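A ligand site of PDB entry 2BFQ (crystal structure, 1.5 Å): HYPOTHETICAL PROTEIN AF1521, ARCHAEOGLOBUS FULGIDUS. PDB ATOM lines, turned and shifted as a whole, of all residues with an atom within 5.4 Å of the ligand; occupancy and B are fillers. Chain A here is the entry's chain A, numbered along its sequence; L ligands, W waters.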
ATOM      1  N   GLY A  19     -15.334   4.548 -32.668  1.00  0.00           N
ATOM      2  CA  GLY A  19     -16.135   4.984 -31.541  1.00  0.00           C
ATOM      3  C   GLY A  19     -15.273   5.139 -30.294  1.00  0.00           C
ATOM      4  O   GLY A  19     -14.038   5.160 -30.371  1.00  0.00           O
ATOM      5  N   ASP A  20     -15.948   5.224 -29.166  1.00  0.00           N
ATOM      6  CA  ASP A  20     -15.337   5.402 -27.852  1.00  0.00           C
ATOM      7  C   ASP A  20     -15.170   4.015 -27.238  1.00  0.00           C
ATOM      8  O   ASP A  20     -16.173   3.302 -27.063  1.00  0.00           O
ATOM      9  CB  ASP A  20     -16.309   6.244 -27.024  1.00  0.00           C
ATOM     10  CG  ASP A  20     -15.813   6.537 -25.630  1.00  0.00           C
ATOM     11  OD1 ASP A  20     -16.452   7.418 -25.004  1.00  0.00           O
ATOM     12  OD2 ASP A  20     -14.832   5.951 -25.140  1.00  0.00           O
ATOM     13  N   ILE A  21     -13.924   3.634 -26.906  1.00  0.00           N
ATOM     14  CA  ILE A  21     -13.670   2.313 -26.362  1.00  0.00           C
ATOM     15  C   ILE A  21     -14.431   2.041 -25.072  1.00  0.00           C
ATOM     16  O   ILE A  21     -14.751   0.890 -24.811  1.00  0.00           O
ATOM     17  CB  ILE A  21     -12.136   2.077 -26.185  1.00  0.00           C
ATOM     18  CG1 ILE A  21     -11.866   0.571 -26.047  1.00  0.00           C
ATOM     19  CG2 ILE A  21     -11.561   2.892 -25.011  1.00  0.00           C
ATOM     20  CD1 ILE A  21     -10.396   0.232 -26.066  1.00  0.00           C
ATOM     21  N   THR A  22     -14.787   3.082 -24.316  1.00  0.00           N
ATOM     22  CA  THR A  22     -15.522   2.864 -23.079  1.00  0.00           C
ATOM     23  C   THR A  22     -16.964   2.441 -23.329  1.00  0.00           C
ATOM     24  O   THR A  22     -17.693   2.149 -22.370  1.00  0.00           O
ATOM     25  CB  THR A  22     -15.514   4.101 -22.161  1.00  0.00           C
ATOM     26  OG1 THR A  22     -16.192   5.205 -22.808  1.00  0.00           O
ATOM     27  CG2 THR A  22     -14.097   4.486 -21.808  1.00  0.00           C
ATOM     28  N   ALA A  32      -4.145   2.561 -23.141  1.00  0.00           N
ATOM     29  CA  ALA A  32      -2.835   2.966 -23.658  1.00  0.00           C
ATOM     30  C   ALA A  32      -2.271   3.874 -22.539  1.00  0.00           C
ATOM     31  O   ALA A  32      -2.446   5.112 -22.525  1.00  0.00           O
ATOM     32  CB  ALA A  32      -3.001   3.738 -24.977  1.00  0.00           C
ATOM     33  N   ALA A  33      -1.577   3.254 -21.605  1.00  0.00           N
ATOM     34  CA  ALA A  33      -1.101   3.967 -20.445  1.00  0.00           C
ATOM     35  C   ALA A  33       0.346   4.387 -20.545  1.00  0.00           C
ATOM     36  O   ALA A  33       1.027   4.087 -21.502  1.00  0.00           O
ATOM     37  CB  ALA A  33      -1.274   3.029 -19.210  1.00  0.00           C
ATOM     38  N   ASN A  34       0.792   5.149 -19.530  1.00  0.00           N
ATOM     39  CA  ASN A  34       2.218   5.423 -19.443  1.00  0.00           C
ATOM     40  C   ASN A  34       2.697   4.420 -18.387  1.00  0.00           C
ATOM     41  O   ASN A  34       1.878   3.753 -17.722  1.00  0.00           O
ATOM     42  CB  ASN A  34       2.515   6.897 -19.050  1.00  0.00           C
ATOM     43  CG  ASN A  34       1.808   7.344 -17.797  1.00  0.00           C
ATOM     44  OD1 ASN A  34       1.967   6.718 -16.733  1.00  0.00           O
ATOM     45  ND2 ASN A  34       1.008   8.384 -17.906  1.00  0.00           N
ATOM     46  N   ARG A  36       3.761   4.609 -15.485  1.00  0.00           N
ATOM     47  CA  ARG A  36       3.403   4.883 -14.091  1.00  0.00           C
ATOM     48  C   ARG A  36       1.901   4.770 -13.862  1.00  0.00           C
ATOM     49  O   ARG A  36       1.420   4.939 -12.728  1.00  0.00           O
ATOM     50  CB  ARG A  36       3.793   6.313 -13.710  1.00  0.00           C
ATOM     51  CG  ARG A  36       5.243   6.707 -14.014  1.00  0.00           C
ATOM     52  CD  ARG A  36       5.431   8.241 -13.929  1.00  0.00           C
ATOM     53  NE  ARG A  36       4.707   8.959 -14.986  1.00  0.00           N
ATOM     54  CZ  ARG A  36       5.062   8.978 -16.273  1.00  0.00           C
ATOM     55  NH1 ARG A  36       4.337   9.640 -17.158  1.00  0.00           N
ATOM     56  NH2 ARG A  36       6.146   8.320 -16.672  1.00  0.00           N
ATOM     57  N   GLU A  38      -0.365   6.849 -14.676  1.00  0.00           N
ATOM     58  CA  GLU A  38      -0.899   8.165 -14.298  1.00  0.00           C
ATOM     59  C   GLU A  38      -1.798   8.559 -15.473  1.00  0.00           C
ATOM     60  O   GLU A  38      -1.307   9.032 -16.505  1.00  0.00           O
ATOM     61  CB  GLU A  38       0.257   9.160 -14.095  1.00  0.00           C
ATOM     62  CG  GLU A  38       1.057   8.862 -12.808  1.00  0.00           C
ATOM     63  CD  GLU A  38       2.279   9.774 -12.615  1.00  0.00           C
ATOM     64  OE1 GLU A  38       2.466  10.730 -13.406  1.00  0.00           O
ATOM     65  OE2 GLU A  38       3.052   9.524 -11.659  1.00  0.00           O
ATOM     66  N   HIS A  39      -3.097   8.411 -15.324  1.00  0.00           N
ATOM     67  CA  HIS A  39      -4.026   8.625 -16.459  1.00  0.00           C
ATOM     68  C   HIS A  39      -4.396  10.081 -16.710  1.00  0.00           C
ATOM     69  O   HIS A  39      -5.525  10.517 -16.433  1.00  0.00           O
ATOM     70  CB  HIS A  39      -5.282   7.780 -16.226  1.00  0.00           C
ATOM     71  CG  HIS A  39      -4.991   6.364 -15.831  1.00  0.00           C
ATOM     72  ND1 HIS A  39      -4.086   5.554 -16.499  1.00  0.00           N
ATOM     73  CD2 HIS A  39      -5.508   5.607 -14.832  1.00  0.00           C
ATOM     74  CE1 HIS A  39      -4.058   4.361 -15.919  1.00  0.00           C
ATOM     75  NE2 HIS A  39      -4.911   4.375 -14.904  1.00  0.00           N
ATOM     76  N   GLY A  40      -3.459  10.769 -17.335  1.00  0.00           N
ATOM     77  CA  GLY A  40      -3.600  12.214 -17.579  1.00  0.00           C
ATOM     78  C   GLY A  40      -4.428  12.723 -18.738  1.00  0.00           C
ATOM     79  O   GLY A  40      -5.003  13.809 -18.624  1.00  0.00           O
ATOM     80  N   GLY A  41      -4.468  11.985 -19.843  1.00  0.00           N
ATOM     81  CA  GLY A  41      -5.237  12.401 -21.005  1.00  0.00           C
ATOM     82  C   GLY A  41      -5.509  11.269 -21.968  1.00  0.00           C
ATOM     83  O   GLY A  41      -5.361  10.089 -21.626  1.00  0.00           O
ATOM     84  N   GLY A  42      -5.923  11.613 -23.179  1.00  0.00           N
ATOM     85  CA  GLY A  42      -6.175  10.599 -24.175  1.00  0.00           C
ATOM     86  C   GLY A  42      -7.106   9.487 -23.713  1.00  0.00           C
ATOM     87  O   GLY A  42      -8.015   9.706 -22.902  1.00  0.00           O
ATOM     88  N   VAL A  43      -6.889   8.292 -24.251  1.00  0.00           N
ATOM     89  CA  VAL A  43      -7.796   7.218 -23.891  1.00  0.00           C
ATOM     90  C   VAL A  43      -7.624   6.842 -22.418  1.00  0.00           C
ATOM     91  O   VAL A  43      -8.635   6.427 -21.822  1.00  0.00           O
ATOM     92  CB  VAL A  43      -7.588   6.013 -24.831  1.00  0.00           C
ATOM     93  CG1 VAL A  43      -6.248   5.354 -24.589  1.00  0.00           C
ATOM     94  CG2 VAL A  43      -8.796   5.033 -24.690  1.00  0.00           C
ATOM     95  N   ALA A  44      -6.442   7.015 -21.832  1.00  0.00           N
ATOM     96  CA  ALA A  44      -6.281   6.703 -20.411  1.00  0.00           C
ATOM     97  C   ALA A  44      -7.241   7.566 -19.570  1.00  0.00           C
ATOM     98  O   ALA A  44      -7.922   7.077 -18.659  1.00  0.00           O
ATOM     99  CB  ALA A  44      -4.868   6.888 -19.963  1.00  0.00           C
ATOM    100  N   ALA A  46     -10.067   9.023 -20.582  1.00  0.00           N
ATOM    101  CA  ALA A  46     -11.400   8.642 -20.925  1.00  0.00           C
ATOM    102  C   ALA A  46     -11.812   7.408 -20.135  1.00  0.00           C
ATOM    103  O   ALA A  46     -12.913   7.341 -19.584  1.00  0.00           O
ATOM    104  CB  ALA A  46     -11.508   8.366 -22.411  1.00  0.00           C
ATOM    105  N   PRO A 138      -7.333   0.127 -28.118  1.00  0.00           N
ATOM    106  CA  PRO A 138      -7.280   1.450 -28.747  1.00  0.00           C
ATOM    107  C   PRO A 138      -5.957   1.353 -29.545  1.00  0.00           C
ATOM    108  O   PRO A 138      -5.179   0.370 -29.454  1.00  0.00           O
ATOM    109  CB  PRO A 138      -7.122   2.392 -27.560  1.00  0.00           C
ATOM    110  CG  PRO A 138      -6.228   1.622 -26.648  1.00  0.00           C
ATOM    111  CD  PRO A 138      -6.635   0.143 -26.824  1.00  0.00           C
ATOM    112  N   ALA A 139      -5.680   2.408 -30.323  1.00  0.00           N
ATOM    113  CA  ALA A 139      -4.457   2.456 -31.122  1.00  0.00           C
ATOM    114  C   ALA A 139      -3.321   2.938 -30.234  1.00  0.00           C
ATOM    115  O   ALA A 139      -2.938   4.130 -30.255  1.00  0.00           O
ATOM    116  CB  ALA A 139      -4.640   3.412 -32.308  1.00  0.00           C
ATOM    117  N   VAL A 140      -2.798   2.008 -29.433  1.00  0.00           N
ATOM    118  CA  VAL A 140      -1.707   2.268 -28.495  1.00  0.00           C
ATOM    119  C   VAL A 140      -0.533   2.996 -29.189  1.00  0.00           C
ATOM    120  O   VAL A 140      -0.134   2.586 -30.254  1.00  0.00           O
ATOM    121  CB  VAL A 140      -1.185   0.941 -27.911  1.00  0.00           C
ATOM    122  CG1 VAL A 140      -0.012   1.213 -26.993  1.00  0.00           C
ATOM    123  CG2 VAL A 140      -2.324   0.242 -27.115  1.00  0.00           C
ATOM    124  N   SER A 141      -0.037   4.054 -28.535  1.00  0.00           N
ATOM    125  CA  SER A 141       1.077   4.895 -29.014  1.00  0.00           C
ATOM    126  C   SER A 141       0.770   5.808 -30.181  1.00  0.00           C
ATOM    127  O   SER A 141       1.671   6.603 -30.587  1.00  0.00           O
ATOM    128  CB  SER A 141       2.300   4.063 -29.353  1.00  0.00           C
ATOM    129  OG  SER A 141       2.888   3.504 -28.181  1.00  0.00           O
ATOM    130  N   ALA A 142      -0.443   5.760 -30.722  1.00  0.00           N
ATOM    131  CA  ALA A 142      -0.761   6.591 -31.895  1.00  0.00           C
ATOM    132  C   ALA A 142      -1.196   7.995 -31.574  1.00  0.00           C
ATOM    133  O   ALA A 142      -1.401   8.821 -32.489  1.00  0.00           O
ATOM    134  CB  ALA A 142      -1.820   5.931 -32.738  1.00  0.00           C
ATOM    135  N   GLY A 143      -1.326   8.284 -30.291  1.00  0.00           N
ATOM    136  CA  GLY A 143      -1.759   9.608 -29.867  1.00  0.00           C
ATOM    137  C   GLY A 143      -0.592  10.482 -29.453  1.00  0.00           C
ATOM    138  O   GLY A 143       0.289  10.802 -30.277  1.00  0.00           O
ATOM    139  N   ILE A 144      -0.548  10.879 -28.191  1.00  0.00           N
ATOM    140  CA  ILE A 144       0.571  11.749 -27.833  1.00  0.00           C
ATOM    141  C   ILE A 144       1.943  11.061 -27.879  1.00  0.00           C
ATOM    142  O   ILE A 144       2.989  11.742 -27.887  1.00  0.00           O
ATOM    143  CB  ILE A 144       0.393  12.450 -26.499  1.00  0.00           C
ATOM    144  CG1 ILE A 144       0.431  11.435 -25.373  1.00  0.00           C
ATOM    145  CG2 ILE A 144      -0.914  13.254 -26.496  1.00  0.00           C
ATOM    146  CD1 ILE A 144       0.437  12.103 -24.012  1.00  0.00           C
ATOM    147  N   TYR A 145       1.986   9.724 -27.911  1.00  0.00           N
ATOM    148  CA  TYR A 145       3.272   9.047 -28.018  1.00  0.00           C
ATOM    149  C   TYR A 145       3.822   9.090 -29.464  1.00  0.00           C
ATOM    150  O   TYR A 145       4.920   8.620 -29.734  1.00  0.00           O
ATOM    151  CB  TYR A 145       3.167   7.623 -27.461  1.00  0.00           C
ATOM    152  CG  TYR A 145       3.346   7.576 -25.956  1.00  0.00           C
ATOM    153  CD1 TYR A 145       3.435   8.748 -25.200  1.00  0.00           C
ATOM    154  CD2 TYR A 145       3.415   6.350 -25.296  1.00  0.00           C
ATOM    155  CE1 TYR A 145       3.595   8.690 -23.810  1.00  0.00           C
ATOM    156  CE2 TYR A 145       3.572   6.274 -23.919  1.00  0.00           C
ATOM    157  CZ  TYR A 145       3.671   7.448 -23.175  1.00  0.00           C
ATOM    158  OH  TYR A 145       3.876   7.364 -21.813  1.00  0.00           O
ATOM    159  N   GLY A 146       3.010   9.624 -30.373  1.00  0.00           N
ATOM    160  CA  GLY A 146       3.469   9.907 -31.730  1.00  0.00           C
ATOM    161  C   GLY A 146       3.929   8.857 -32.687  1.00  0.00           C
ATOM    162  O   GLY A 146       4.801   9.097 -33.551  1.00  0.00           O
ATOM    163  N   LEU A 149       0.109   6.063 -37.229  1.00  0.00           N
ATOM    164  CA  LEU A 149      -1.059   5.208 -37.121  1.00  0.00           C
ATOM    165  C   LEU A 149      -0.989   3.950 -37.970  1.00  0.00           C
ATOM    166  O   LEU A 149      -1.341   2.874 -37.515  1.00  0.00           O
ATOM    167  CB  LEU A 149      -2.339   5.975 -37.447  1.00  0.00           C
ATOM    168  CG  LEU A 149      -3.646   5.190 -37.286  1.00  0.00           C
ATOM    169  CD1 LEU A 149      -3.762   4.675 -35.852  1.00  0.00           C
ATOM    170  CD2 LEU A 149      -4.847   6.065 -37.652  1.00  0.00           C
ATOM    171  N   VAL A 174     -10.525  -0.337 -31.658  1.00  0.00           N
ATOM    172  CA  VAL A 174     -11.469   0.780 -31.671  1.00  0.00           C
ATOM    173  C   VAL A 174     -10.698   2.067 -31.916  1.00  0.00           C
ATOM    174  O   VAL A 174      -9.834   2.437 -31.126  1.00  0.00           O
ATOM    175  CB  VAL A 174     -12.225   0.865 -30.316  1.00  0.00           C
ATOM    176  CG1 VAL A 174     -13.297   1.983 -30.352  1.00  0.00           C
ATOM    177  CG2 VAL A 174     -12.852  -0.471 -30.012  1.00  0.00           C
ATOM    178  N   ILE A 175     -11.037   2.748 -33.016  1.00  0.00           N
ATOM    179  CA  ILE A 175     -10.387   3.987 -33.405  1.00  0.00           C
ATOM    180  C   ILE A 175     -11.360   5.125 -33.138  1.00  0.00           C
ATOM    181  O   ILE A 175     -12.543   5.047 -33.471  1.00  0.00           O
ATOM    182  CB  ILE A 175      -9.980   3.937 -34.900  1.00  0.00           C
ATOM    183  CG1 ILE A 175      -9.018   2.772 -35.173  1.00  0.00           C
ATOM    184  CG2 ILE A 175      -9.374   5.268 -35.328  1.00  0.00           C
ATOM    185  CD1 ILE A 175      -7.707   2.807 -34.424  1.00  0.00           C
ATOM    186  N   TYR A 176     -10.842   6.194 -32.554  1.00  0.00           N
ATOM    187  CA  TYR A 176     -11.652   7.329 -32.123  1.00  0.00           C
ATOM    188  C   TYR A 176     -12.156   8.330 -33.138  1.00  0.00           C
ATOM    189  O   TYR A 176     -13.364   8.572 -33.241  1.00  0.00           O
ATOM    190  CB  TYR A 176     -10.892   8.075 -31.047  1.00  0.00           C
ATOM    191  CG  TYR A 176     -11.737   8.875 -30.113  1.00  0.00           C
ATOM    192  CD1 TYR A 176     -12.879   8.332 -29.530  1.00  0.00           C
ATOM    193  CD2 TYR A 176     -11.361  10.182 -29.754  1.00  0.00           C
ATOM    194  CE1 TYR A 176     -13.626   9.052 -28.610  1.00  0.00           C
ATOM    195  CE2 TYR A 176     -12.108  10.902 -28.834  1.00  0.00           C
ATOM    196  CZ  TYR A 176     -13.240  10.336 -28.269  1.00  0.00           C
ATOM    197  OH  TYR A 176     -13.974  11.047 -27.347  1.00  0.00           O
ATOM    198  N   ASP A 177     -11.242   8.956 -33.851  1.00  0.00           N
ATOM    199  CA  ASP A 177     -11.670   9.973 -34.809  1.00  0.00           C
ATOM    200  C   ASP A 177     -11.846   9.388 -36.200  1.00  0.00           C
ATOM    201  O   ASP A 177     -11.232   8.383 -36.549  1.00  0.00           O
ATOM    202  CB  ASP A 177     -10.678  11.148 -34.805  1.00  0.00           C
ATOM    203  CG  ASP A 177      -9.410  10.853 -35.557  1.00  0.00           C
ATOM    204  OD1 ASP A 177      -9.412  10.949 -36.803  1.00  0.00           O
ATOM    205  OD2 ASP A 177      -8.390  10.524 -34.906  1.00  0.00           O
ATOM    206  N   SER A 180      -8.685   8.999 -38.658  1.00  0.00           N
ATOM    207  CA  SER A 180      -7.878   7.859 -38.249  1.00  0.00           C
ATOM    208  C   SER A 180      -8.526   6.524 -38.572  1.00  0.00           C
ATOM    209  O   SER A 180      -7.846   5.577 -38.956  1.00  0.00           O
ATOM    210  CB  SER A 180      -7.612   7.921 -36.747  1.00  0.00           C
ATOM    211  OG  SER A 180      -6.918   9.104 -36.392  1.00  0.00           O
HETATM  212  N1  LIG L   1     -11.669   5.563 -27.324  1.00  0.00           N
HETATM  213  C1  LIG L   1     -10.804   5.043 -28.276  1.00  0.00           C
HETATM  214  N2  LIG L   1      -9.700   5.724 -28.643  1.00  0.00           N
HETATM  215  C2  LIG L   1      -9.430   6.934 -28.070  1.00  0.00           C
HETATM  216  C3  LIG L   1     -10.254   7.486 -27.117  1.00  0.00           C
HETATM  217  C4  LIG L   1     -11.436   6.775 -26.706  1.00  0.00           C
HETATM  218  N3  LIG L   1     -12.262   7.232 -25.806  1.00  0.00           N
HETATM  219  N4  LIG L   1      -9.705   8.681 -26.760  1.00  0.00           N
HETATM  220  C5  LIG L   1      -8.583   8.785 -27.499  1.00  0.00           C
HETATM  221  N5  LIG L   1      -8.353   7.722 -28.331  1.00  0.00           N
HETATM  222  P1  LIG L   1      -3.253   8.307 -26.522  1.00  0.00           P
HETATM  223  P2  LIG L   1      -0.645   7.129 -26.409  1.00  0.00           P
HETATM  224  C6  LIG L   1      -7.296   7.344 -29.285  1.00  0.00           C
HETATM  225  O1  LIG L   1      -4.416   8.186 -25.563  1.00  0.00           O
HETATM  226  O2  LIG L   1      -0.200   7.723 -27.756  1.00  0.00           O
HETATM  227  C7  LIG L   1      -1.990   9.427 -21.902  1.00  0.00           C
HETATM  228  O3  LIG L   1      -1.898  10.761 -21.329  1.00  0.00           O
HETATM  229  C8  LIG L   1      -6.481   8.524 -29.848  1.00  0.00           C
HETATM  230  O4  LIG L   1      -7.187   9.314 -30.797  1.00  0.00           O
HETATM  231  O5  LIG L   1      -2.648   9.729 -26.537  1.00  0.00           O
HETATM  232  O6  LIG L   1      -0.268   5.696 -26.217  1.00  0.00           O
HETATM  233  C9  LIG L   1      -1.484   8.331 -21.003  1.00  0.00           C
HETATM  234  O7  LIG L   1      -1.741   8.454 -19.600  1.00  0.00           O
HETATM  235  C10 LIG L   1      -5.256   7.768 -30.333  1.00  0.00           C
HETATM  236  O8  LIG L   1      -5.408   7.332 -31.675  1.00  0.00           O
HETATM  237  O9  LIG L   1      -2.196   7.269 -26.117  1.00  0.00           O
HETATM  238  C11 LIG L   1      -0.014   8.310 -21.406  1.00  0.00           C
HETATM  239  O10 LIG L   1       0.795   9.210 -20.666  1.00  0.00           O
HETATM  240  C12 LIG L   1      -5.114   6.550 -29.385  1.00  0.00           C
HETATM  241  O11 LIG L   1      -6.332   6.576 -28.609  1.00  0.00           O
HETATM  242  C13 LIG L   1       0.035   8.513 -22.910  1.00  0.00           C
HETATM  243  O12 LIG L   1      -1.141   9.366 -23.048  1.00  0.00           O
HETATM  244  C14 LIG L   1      -3.988   6.622 -28.362  1.00  0.00           C
HETATM  245  O13 LIG L   1      -3.783   8.025 -27.950  1.00  0.00           O
HETATM  246  C15 LIG L   1      -0.054   7.356 -23.891  1.00  0.00           C
HETATM  247  O14 LIG L   1      -0.073   7.947 -25.207  1.00  0.00           O
HETATM  248  O   HOH W   1      -6.984  11.564 -27.942  1.00  0.00           O
HETATM  249  O   HOH W   2     -11.052  10.829 -25.743  1.00  0.00           O
HETATM  250  O   HOH W   3      -4.211  11.810 -27.568  1.00  0.00           O
HETATM  251  O   HOH W   4      -7.960   4.180 -30.469  1.00  0.00           O
HETATM  252  O   HOH W   5      -4.281   9.248 -33.260  1.00  0.00           O
HETATM  253  O   HOH W   6       0.713   3.648 -24.313  1.00  0.00           O
HETATM  254  O   HOH W   7      -7.729   5.992 -32.514  1.00  0.00           O
HETATM  255  O   HOH W   8      -3.219  11.233 -24.272  1.00  0.00           O
HETATM  256  O   HOH W   9     -13.643  10.083 -24.721  1.00  0.00           O
HETATM  257  O   HOH W  10      -4.008   7.321 -23.069  1.00  0.00           O
HETATM  258  O   HOH W  11      -7.616  11.887 -30.647  1.00  0.00           O
HETATM  259  O   HOH W  12      -1.577   6.166 -17.908  1.00  0.00           O
HETATM  260  O   HOH W  13      -0.847  10.947 -18.550  1.00  0.00           O
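N of Ile 21 lies within hydrogen-bond range of N1 of the ligand (3.0 Å).
The backbone NH (N) of Ser 141 is in hydrogen-bond range of an oxygen (O6) of the ligand.
N of Val 43 lies within hydrogen-bond range of O1 of the ligand (2.8 Å).
The backbone NH (N) of Gly 41 lies within hydrogen-bond range of an oxygen (O3) of the ligand.
O2 of the ligand is in hydrogen-bond range of N of Gly 143 (2.8 Å).
O7 of the ligand sits at hydrogen-bond distance from O of Glu 38 (3.2 Å).
The side-chain carboxylate (OD2) of Asp 20 sits at hydrogen-bond distance from a nitrogen (N3) of the ligand, 2.9 Å away.
N of Tyr 145 sits at hydrogen-bond distance from O2 of the ligand (3.0 Å).
O5 of the ligand lies within hydrogen-bond range of N of Ile 144 (2.9 Å).
An oxygen (O10) of the ligand is in hydrogen-bond range of the side-chain amide nitrogen (ND2) of Asn 34, at 2.9 Å.
Merely in contact with the ligand: Gly 42, Ala 139, Tyr 176, Ala 44, Ala 32, Ala 142, Ala 46, Gly 40, Gly 19, His 39 and Val 174.
Hydrophobic or aromatic side chains that line the ligand: Ile 21, Ala 32, Val 43, Ala 44, Ala 46, Ala 142, Ile 144, Tyr 145 and Tyr 176.
Within 4 Å of the ligand: Gly 19, Asp 20, Ile 21, Ala 32, Asn 34, Glu 38, His 39, Gly 40, Gly 41, Gly 42, Val 43, Ala 44, Ala 46, Ala 139, Ser 141, Ala 142, Gly 143, Ile 144, Tyr 145, Val 174 and Tyr 176.
Water W5 bridges an oxygen (O8) of the ligand (2.7 Å) and the backbone carbonyl oxygen (O) of Ala 142 (3.0 Å).
Water W2 bridges a nitrogen (N4) of the ligand (2.7 Å) and the side-chain hydroxyl of Tyr 176 (3.3 Å).
Water W8 bridges O5 of the ligand (2.8 Å) and N of Gly 42 (2.9 Å).
Water W7 lies within hydrogen-bond range of an oxygen (O8) of the ligand and the backbone NH of Tyr 176.
Water W12 lies within hydrogen-bond range of O7 of the ligand (2.9 Å), ND1 of His 39 (2.9 Å), N of Asn 34 (3.0 Å) and O of Glu 38 (3.2 Å).
Water W9 lies within hydrogen-bond range of the side-chain hydroxyl (OH) of Tyr 176 and a nitrogen (N3) of the ligand.
The backbone carbonyl oxygen (O) of Glu 38 is in hydrogen-bond range of the side-chain amide nitrogen (ND2) of Asn 34 (2.8 Å).
The backbone NH (N) of Gly 146 lies within hydrogen-bond range of the backbone carbonyl oxygen (O) of Ser 141 (3.3 Å).
The side-chain amide oxygen of Asn 34 is in hydrogen-bond range of the backbone NH of Arg 36, at 3.0 Å.
The side-chain carboxylate of Asp 20 is in hydrogen-bond range of the side-chain hydroxyl of Thr 22.
N of Gly 19 sits at hydrogen-bond distance from O of Ile 175, 2.9 Å away.
The side-chain carboxylate (OE1) of Glu 38 lies within salt-bridge range of the guanidinium group (NE) of Arg 36 (3.3 Å).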
